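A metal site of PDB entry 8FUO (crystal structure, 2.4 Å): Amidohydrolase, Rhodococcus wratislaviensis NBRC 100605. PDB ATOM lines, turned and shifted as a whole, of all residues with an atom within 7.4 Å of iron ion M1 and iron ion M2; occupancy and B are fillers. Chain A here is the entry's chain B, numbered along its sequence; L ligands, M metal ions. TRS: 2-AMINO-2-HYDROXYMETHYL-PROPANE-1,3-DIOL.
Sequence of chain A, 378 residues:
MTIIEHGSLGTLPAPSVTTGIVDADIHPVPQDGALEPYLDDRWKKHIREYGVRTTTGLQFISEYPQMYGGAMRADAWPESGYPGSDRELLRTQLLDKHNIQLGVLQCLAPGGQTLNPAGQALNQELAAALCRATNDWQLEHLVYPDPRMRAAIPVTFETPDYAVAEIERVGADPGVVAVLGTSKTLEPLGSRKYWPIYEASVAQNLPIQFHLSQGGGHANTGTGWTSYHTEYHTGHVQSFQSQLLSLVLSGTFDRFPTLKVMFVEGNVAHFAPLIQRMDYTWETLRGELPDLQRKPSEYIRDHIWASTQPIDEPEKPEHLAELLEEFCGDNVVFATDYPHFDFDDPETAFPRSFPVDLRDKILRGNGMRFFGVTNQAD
N of His 27 lies within hydrogen-bond range of O of Tyr 338 (2.9 Å). The backbone NH (N) of Glu 265 sits at hydrogen-bond distance from the side-chain hydroxyl (OG) of Ser 307, at 3.1 Å. OD2 of Asp 337 sits close to OE1 of Gln 309, 3.4 Å away. ND1 of His 27 is in hydrogen-bond range of O of Gln 106. The side-chain amide oxygen of Gln 309 sits close to the side-chain carboxylate of Glu 265, 3.5 Å away. The side-chain carboxylate of Asp 25 lies close to the side-chain amide oxygen of Gln 106 (3.0 Å).
Along chain A the residues within 4 Å of iron ion M2 span positions 265 to 340. The nearest printed residue that does not touch iron ion M2 is His 27 (4.2 Å).
Iron ion M1 is bound by OD1 of Asp 337, NE2 of His 27, OE1 of Glu 265, OD2 of Asp 25 and NE2 of His 211. Iron ion M1 has five donor atoms within binding distance.
OE2 of Glu 265 binds iron ion M2. OD2 of Asp 337 is bound to iron ion M2 (2.2 Å). Iron ion M2 is bound by ND1 of His 340 (2.3 Å). Iron ion M2 is bound by N of the ligand. O3 of the ligand is bound to iron ion M2, 2.3 Å away.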
ATOM      1  N   ASP A  25       4.475  13.707  26.279  1.00  0.00           N
ATOM      2  CA  ASP A  25       3.497  12.876  25.601  1.00  0.00           C
ATOM      3  C   ASP A  25       3.871  12.745  24.121  1.00  0.00           C
ATOM      4  O   ASP A  25       3.627  13.654  23.322  1.00  0.00           O
ATOM      5  CB  ASP A  25       2.077  13.453  25.747  1.00  0.00           C
ATOM      6  CG  ASP A  25       1.039  12.545  25.172  1.00  0.00           C
ATOM      7  OD1 ASP A  25       1.161  11.351  25.381  1.00  0.00           O
ATOM      8  OD2 ASP A  25       0.117  13.016  24.473  1.00  0.00           O
ATOM      9  N   ILE A  26       4.398  11.562  23.768  1.00  0.00           N
ATOM     10  CA  ILE A  26       4.809  11.188  22.413  1.00  0.00           C
ATOM     11  C   ILE A  26       4.254   9.808  22.129  1.00  0.00           C
ATOM     12  O   ILE A  26       4.356   8.910  22.970  1.00  0.00           O
ATOM     13  CB  ILE A  26       6.340  11.139  22.263  1.00  0.00           C
ATOM     14  CG1 ILE A  26       6.975  12.501  22.467  1.00  0.00           C
ATOM     15  CG2 ILE A  26       6.750  10.535  20.911  1.00  0.00           C
ATOM     16  CD1 ILE A  26       8.416  12.380  22.846  1.00  0.00           C
ATOM     17  N   HIS A  27       3.716   9.620  20.917  1.00  0.00           N
ATOM     18  CA  HIS A  27       2.986   8.407  20.558  1.00  0.00           C
ATOM     19  C   HIS A  27       3.731   7.578  19.509  1.00  0.00           C
ATOM     20  O   HIS A  27       3.476   7.730  18.289  1.00  0.00           O
ATOM     21  CB  HIS A  27       1.580   8.779  20.082  1.00  0.00           C
ATOM     22  CG  HIS A  27       0.742   9.365  21.163  1.00  0.00           C
ATOM     23  ND1 HIS A  27       0.647   8.789  22.411  1.00  0.00           N
ATOM     24  CD2 HIS A  27       0.009  10.508  21.231  1.00  0.00           C
ATOM     25  CE1 HIS A  27      -0.132   9.526  23.182  1.00  0.00           C
ATOM     26  NE2 HIS A  27      -0.530  10.576  22.484  1.00  0.00           N
ATOM     27  N   ALA A  71      -6.105  11.483  12.305  1.00  0.00           N
ATOM     28  CA  ALA A  71      -5.855  12.539  13.241  1.00  0.00           C
ATOM     29  C   ALA A  71      -4.384  12.687  13.362  1.00  0.00           C
ATOM     30  O   ALA A  71      -3.892  13.081  14.367  1.00  0.00           O
ATOM     31  CB  ALA A  71      -6.556  12.358  14.560  1.00  0.00           C
ATOM     32  N   GLN A 106       4.166   7.283  25.211  1.00  0.00           N
ATOM     33  CA  GLN A 106       2.844   6.812  25.632  1.00  0.00           C
ATOM     34  C   GLN A 106       2.252   6.086  24.428  1.00  0.00           C
ATOM     35  O   GLN A 106       1.530   6.655  23.601  1.00  0.00           O
ATOM     36  CB  GLN A 106       1.947   7.958  26.145  1.00  0.00           C
ATOM     37  CG  GLN A 106       2.660   8.896  27.112  1.00  0.00           C
ATOM     38  CD  GLN A 106       1.712   9.758  27.931  1.00  0.00           C
ATOM     39  OE1 GLN A 106       0.497   9.665  27.784  1.00  0.00           O
ATOM     40  NE2 GLN A 106       2.260  10.619  28.788  1.00  0.00           N
ATOM     41  N   LEU A 108      -0.191   4.107  22.493  1.00  0.00           N
ATOM     42  CA  LEU A 108      -1.636   4.062  22.671  1.00  0.00           C
ATOM     43  C   LEU A 108      -2.304   2.868  21.982  1.00  0.00           C
ATOM     44  O   LEU A 108      -3.515   2.702  22.132  1.00  0.00           O
ATOM     45  CB  LEU A 108      -2.268   5.345  22.119  1.00  0.00           C
ATOM     46  CG  LEU A 108      -2.063   6.690  22.823  1.00  0.00           C
ATOM     47  CD1 LEU A 108      -2.988   7.711  22.158  1.00  0.00           C
ATOM     48  CD2 LEU A 108      -2.267   6.626  24.366  1.00  0.00           C
ATOM     49  N   THR A 114      -4.374   4.583  15.784  1.00  0.00           N
ATOM     50  CA  THR A 114      -4.140   5.833  16.501  1.00  0.00           C
ATOM     51  C   THR A 114      -4.372   5.693  18.003  1.00  0.00           C
ATOM     52  O   THR A 114      -3.504   6.065  18.807  1.00  0.00           O
ATOM     53  CB  THR A 114      -5.038   6.934  15.925  1.00  0.00           C
ATOM     54  OG1 THR A 114      -4.705   7.128  14.553  1.00  0.00           O
ATOM     55  CG2 THR A 114      -4.823   8.249  16.679  1.00  0.00           C
ATOM     56  N   LEU A 115      -5.524   5.171  18.402  1.00  0.00           N
ATOM     57  CA  LEU A 115      -5.888   5.056  19.818  1.00  0.00           C
ATOM     58  C   LEU A 115      -6.657   3.745  19.988  1.00  0.00           C
ATOM     59  O   LEU A 115      -7.824   3.660  19.595  1.00  0.00           O
ATOM     60  CB  LEU A 115      -6.711   6.264  20.251  1.00  0.00           C
ATOM     61  CG  LEU A 115      -7.345   6.319  21.648  1.00  0.00           C
ATOM     62  CD1 LEU A 115      -6.299   6.185  22.752  1.00  0.00           C
ATOM     63  CD2 LEU A 115      -8.151   7.619  21.813  1.00  0.00           C
ATOM     64  N   HIS A 211      -3.540   9.237  30.357  1.00  0.00           N
ATOM     65  CA  HIS A 211      -3.767   9.783  29.025  1.00  0.00           C
ATOM     66  C   HIS A 211      -5.232   9.635  28.600  1.00  0.00           C
ATOM     67  O   HIS A 211      -5.925   8.670  28.957  1.00  0.00           O
ATOM     68  CB  HIS A 211      -2.855   9.087  28.008  1.00  0.00           C
ATOM     69  CG  HIS A 211      -2.881   9.718  26.664  1.00  0.00           C
ATOM     70  ND1 HIS A 211      -3.776   9.345  25.671  1.00  0.00           N
ATOM     71  CD2 HIS A 211      -2.120  10.704  26.127  1.00  0.00           C
ATOM     72  CE1 HIS A 211      -3.567  10.079  24.597  1.00  0.00           C
ATOM     73  NE2 HIS A 211      -2.565  10.904  24.844  1.00  0.00           N
ATOM     74  N   LEU A 212      -5.678  10.630  27.841  1.00  0.00           N
ATOM     75  CA  LEU A 212      -6.962  10.626  27.132  1.00  0.00           C
ATOM     76  C   LEU A 212      -7.269   9.279  26.478  1.00  0.00           C
ATOM     77  O   LEU A 212      -6.473   8.765  25.691  1.00  0.00           O
ATOM     78  CB  LEU A 212      -6.909  11.740  26.076  1.00  0.00           C
ATOM     79  CG  LEU A 212      -7.874  12.003  24.914  1.00  0.00           C
ATOM     80  CD1 LEU A 212      -7.619  13.415  24.368  1.00  0.00           C
ATOM     81  CD2 LEU A 212      -7.776  10.985  23.778  1.00  0.00           C
ATOM     82  N   HIS A 233     -14.341  15.172  20.851  1.00  0.00           N
ATOM     83  CA  HIS A 233     -13.020  15.653  21.210  1.00  0.00           C
ATOM     84  C   HIS A 233     -13.098  16.640  22.385  1.00  0.00           C
ATOM     85  O   HIS A 233     -12.307  16.527  23.338  1.00  0.00           O
ATOM     86  CB  HIS A 233     -12.339  16.260  19.973  1.00  0.00           C
ATOM     87  CG  HIS A 233     -10.854  16.360  20.100  1.00  0.00           C
ATOM     88  ND1 HIS A 233     -10.051  16.887  19.097  1.00  0.00           N
ATOM     89  CD2 HIS A 233     -10.011  16.024  21.104  1.00  0.00           C
ATOM     90  CE1 HIS A 233      -8.786  16.864  19.481  1.00  0.00           C
ATOM     91  NE2 HIS A 233      -8.735  16.348  20.696  1.00  0.00           N
ATOM     92  N   VAL A 264      -3.074  13.867  31.293  1.00  0.00           N
ATOM     93  CA  VAL A 264      -2.352  14.090  30.040  1.00  0.00           C
ATOM     94  C   VAL A 264      -3.374  14.239  28.918  1.00  0.00           C
ATOM     95  O   VAL A 264      -4.170  13.325  28.675  1.00  0.00           O
ATOM     96  CB  VAL A 264      -1.367  12.963  29.733  1.00  0.00           C
ATOM     97  CG1 VAL A 264      -0.762  13.130  28.324  1.00  0.00           C
ATOM     98  CG2 VAL A 264      -0.309  12.879  30.815  1.00  0.00           C
ATOM     99  N   GLU A 265      -3.326  15.379  28.233  1.00  0.00           N
ATOM    100  CA  GLU A 265      -4.240  15.694  27.145  1.00  0.00           C
ATOM    101  C   GLU A 265      -5.698  15.773  27.622  1.00  0.00           C
ATOM    102  O   GLU A 265      -6.623  15.366  26.931  1.00  0.00           O
ATOM    103  CB  GLU A 265      -4.091  14.674  26.018  1.00  0.00           C
ATOM    104  CG  GLU A 265      -4.398  15.224  24.678  1.00  0.00           C
ATOM    105  CD  GLU A 265      -3.789  14.365  23.622  1.00  0.00           C
ATOM    106  OE1 GLU A 265      -2.695  13.831  23.894  1.00  0.00           O
ATOM    107  OE2 GLU A 265      -4.414  14.185  22.549  1.00  0.00           O
ATOM    108  N   SER A 307      -0.561  18.091  31.652  1.00  0.00           N
ATOM    109  CA  SER A 307       0.227  18.447  30.481  1.00  0.00           C
ATOM    110  C   SER A 307      -0.533  19.488  29.639  1.00  0.00           C
ATOM    111  O   SER A 307      -1.746  19.659  29.769  1.00  0.00           O
ATOM    112  CB  SER A 307       0.574  17.195  29.685  1.00  0.00           C
ATOM    113  OG  SER A 307      -0.551  16.650  28.999  1.00  0.00           O
ATOM    114  N   GLN A 309      -0.572  20.296  25.995  1.00  0.00           N
ATOM    115  CA  GLN A 309      -1.224  19.988  24.732  1.00  0.00           C
ATOM    116  C   GLN A 309      -2.596  19.364  24.970  1.00  0.00           C
ATOM    117  O   GLN A 309      -2.758  18.539  25.880  1.00  0.00           O
ATOM    118  CB  GLN A 309      -0.326  19.026  23.939  1.00  0.00           C
ATOM    119  CG  GLN A 309      -0.652  18.907  22.475  1.00  0.00           C
ATOM    120  CD  GLN A 309      -1.829  18.000  22.196  1.00  0.00           C
ATOM    121  OE1 GLN A 309      -2.221  17.181  23.027  1.00  0.00           O
ATOM    122  NE2 GLN A 309      -2.394  18.137  20.997  1.00  0.00           N
ATOM    123  N   PRO A 310      -3.634  19.724  24.171  1.00  0.00           N
ATOM    124  CA  PRO A 310      -3.632  20.792  23.147  1.00  0.00           C
ATOM    125  C   PRO A 310      -3.899  22.157  23.799  1.00  0.00           C
ATOM    126  O   PRO A 310      -5.002  22.355  24.328  1.00  0.00           O
ATOM    127  CB  PRO A 310      -4.754  20.377  22.206  1.00  0.00           C
ATOM    128  CG  PRO A 310      -5.731  19.616  23.109  1.00  0.00           C
ATOM    129  CD  PRO A 310      -4.916  18.989  24.190  1.00  0.00           C
ATOM    130  N   ALA A 335       3.922  19.263  26.575  1.00  0.00           N
ATOM    131  CA  ALA A 335       3.864  18.096  25.717  1.00  0.00           C
ATOM    132  C   ALA A 335       3.685  18.553  24.280  1.00  0.00           C
ATOM    133  O   ALA A 335       3.138  19.622  24.021  1.00  0.00           O
ATOM    134  CB  ALA A 335       2.725  17.129  26.114  1.00  0.00           C
ATOM    135  N   THR A 336       4.130  17.722  23.329  1.00  0.00           N
ATOM    136  CA  THR A 336       3.844  17.993  21.929  1.00  0.00           C
ATOM    137  C   THR A 336       2.653  17.213  21.398  1.00  0.00           C
ATOM    138  O   THR A 336       1.944  17.715  20.528  1.00  0.00           O
ATOM    139  CB  THR A 336       5.052  17.692  21.020  1.00  0.00           C
ATOM    140  OG1 THR A 336       5.233  16.266  20.823  1.00  0.00           O
ATOM    141  CG2 THR A 336       6.305  18.343  21.577  1.00  0.00           C
ATOM    142  N   ASP A 337       2.435  15.999  21.901  1.00  0.00           N
ATOM    143  CA  ASP A 337       1.505  15.046  21.323  1.00  0.00           C
ATOM    144  C   ASP A 337       1.914  14.598  19.912  1.00  0.00           C
ATOM    145  O   ASP A 337       1.055  14.216  19.117  1.00  0.00           O
ATOM    146  CB  ASP A 337       0.074  15.605  21.286  1.00  0.00           C
ATOM    147  CG  ASP A 337      -0.963  14.538  21.320  1.00  0.00           C
ATOM    148  OD1 ASP A 337      -0.681  13.496  21.939  1.00  0.00           O
ATOM    149  OD2 ASP A 337      -2.048  14.710  20.728  1.00  0.00           O
ATOM    150  N   TYR A 338       3.199  14.631  19.587  1.00  0.00           N
ATOM    151  CA  TYR A 338       3.636  14.137  18.292  1.00  0.00           C
ATOM    152  C   TYR A 338       3.289  12.653  18.159  1.00  0.00           C
ATOM    153  O   TYR A 338       3.527  11.873  19.090  1.00  0.00           O
ATOM    154  CB  TYR A 338       5.144  14.302  18.128  1.00  0.00           C
ATOM    155  CG  TYR A 338       5.676  13.777  16.806  1.00  0.00           C
ATOM    156  CD1 TYR A 338       5.862  14.628  15.715  1.00  0.00           C
ATOM    157  CD2 TYR A 338       5.999  12.438  16.660  1.00  0.00           C
ATOM    158  CE1 TYR A 338       6.337  14.150  14.512  1.00  0.00           C
ATOM    159  CE2 TYR A 338       6.470  11.944  15.454  1.00  0.00           C
ATOM    160  CZ  TYR A 338       6.644  12.799  14.390  1.00  0.00           C
ATOM    161  OH  TYR A 338       7.125  12.294  13.194  1.00  0.00           O
ATOM    162  N   PRO A 339       2.807  12.195  16.984  1.00  0.00           N
ATOM    163  CA  PRO A 339       2.548  12.874  15.702  1.00  0.00           C
ATOM    164  C   PRO A 339       1.094  13.204  15.425  1.00  0.00           C
ATOM    165  O   PRO A 339       0.659  13.075  14.275  1.00  0.00           O
ATOM    166  CB  PRO A 339       3.031  11.841  14.682  1.00  0.00           C
ATOM    167  CG  PRO A 339       2.644  10.555  15.311  1.00  0.00           C
ATOM    168  CD  PRO A 339       2.774  10.733  16.822  1.00  0.00           C
ATOM    169  N   HIS A 340       0.342  13.609  16.452  1.00  0.00           N
ATOM    170  CA  HIS A 340      -1.072  13.868  16.245  1.00  0.00           C
ATOM    171  C   HIS A 340      -1.276  15.234  15.602  1.00  0.00           C
ATOM    172  O   HIS A 340      -0.402  16.106  15.670  1.00  0.00           O
ATOM    173  CB  HIS A 340      -1.838  13.747  17.559  1.00  0.00           C
ATOM    174  CG  HIS A 340      -1.997  12.339  18.011  1.00  0.00           C
ATOM    175  ND1 HIS A 340      -2.800  11.973  19.063  1.00  0.00           N
ATOM    176  CD2 HIS A 340      -1.464  11.183  17.528  1.00  0.00           C
ATOM    177  CE1 HIS A 340      -2.756  10.651  19.216  1.00  0.00           C
ATOM    178  NE2 HIS A 340      -1.947  10.158  18.295  1.00  0.00           N
ATOM    179  N   PHE A 341      -2.431  15.395  14.966  1.00  0.00           N
ATOM    180  CA  PHE A 341      -2.631  16.534  14.070  1.00  0.00           C
ATOM    181  C   PHE A 341      -2.616  17.858  14.821  1.00  0.00           C
ATOM    182  O   PHE A 341      -2.185  18.878  14.256  1.00  0.00           O
ATOM    183  CB  PHE A 341      -3.932  16.376  13.296  1.00  0.00           C
ATOM    184  CG  PHE A 341      -5.140  16.908  14.028  1.00  0.00           C
ATOM    185  CD1 PHE A 341      -5.828  16.114  14.940  1.00  0.00           C
ATOM    186  CD2 PHE A 341      -5.557  18.216  13.838  1.00  0.00           C
ATOM    187  CE1 PHE A 341      -6.932  16.605  15.626  1.00  0.00           C
ATOM    188  CE2 PHE A 341      -6.650  18.726  14.533  1.00  0.00           C
ATOM    189  CZ  PHE A 341      -7.339  17.922  15.435  1.00  0.00           C
ATOM    190  N   ASP A 342      -3.086  17.883  16.082  1.00  0.00           N
ATOM    191  CA  ASP A 342      -3.050  19.093  16.898  1.00  0.00           C
ATOM    192  C   ASP A 342      -1.747  19.208  17.705  1.00  0.00           C
ATOM    193  O   ASP A 342      -1.699  19.983  18.672  1.00  0.00           O
ATOM    194  CB  ASP A 342      -4.291  19.189  17.816  1.00  0.00           C
ATOM    195  CG  ASP A 342      -4.617  17.886  18.591  1.00  0.00           C
ATOM    196  OD1 ASP A 342      -3.921  16.850  18.387  1.00  0.00           O
ATOM    197  OD2 ASP A 342      -5.588  17.921  19.397  1.00  0.00           O
ATOM    198  N   PHE A 343      -0.697  18.497  17.281  1.00  0.00           N
ATOM    199  CA  PHE A 343       0.674  18.667  17.752  1.00  0.00           C
ATOM    200  C   PHE A 343       0.971  20.088  18.238  1.00  0.00           C
ATOM    201  O   PHE A 343       0.562  21.059  17.592  1.00  0.00           O
ATOM    202  CB  PHE A 343       1.637  18.287  16.620  1.00  0.00           C
ATOM    203  CG  PHE A 343       3.067  18.705  16.842  1.00  0.00           C
ATOM    204  CD1 PHE A 343       3.540  19.925  16.354  1.00  0.00           C
ATOM    205  CD2 PHE A 343       3.971  17.841  17.469  1.00  0.00           C
ATOM    206  CE1 PHE A 343       4.876  20.297  16.530  1.00  0.00           C
ATOM    207  CE2 PHE A 343       5.304  18.207  17.653  1.00  0.00           C
ATOM    208  CZ  PHE A 343       5.748  19.448  17.185  1.00  0.00           C
HETATM  209  C   TRS L   1      -6.358  12.849  19.468  1.00  0.00           C
HETATM  210  C1  TRS L   1      -6.010  11.873  18.349  1.00  0.00           C
HETATM  211  C2  TRS L   1      -7.866  12.834  19.701  1.00  0.00           C
HETATM  212  C3  TRS L   1      -5.913  14.285  19.124  1.00  0.00           C
HETATM  213  N   TRS L   1      -5.736  12.292  20.665  1.00  0.00           N
HETATM  214  O1  TRS L   1      -6.651  10.662  18.690  1.00  0.00           O
HETATM  215  O2  TRS L   1      -8.568  13.120  18.502  1.00  0.00           O
HETATM  216  O3  TRS L   1      -4.534  14.549  19.337  1.00  0.00           O
HETATM  217 FE    FE M   1      -1.531  12.237  23.209  1.00  0.00          FE
HETATM  218 FE    FE M   2      -3.545  13.106  20.905  1.00  0.00          FE
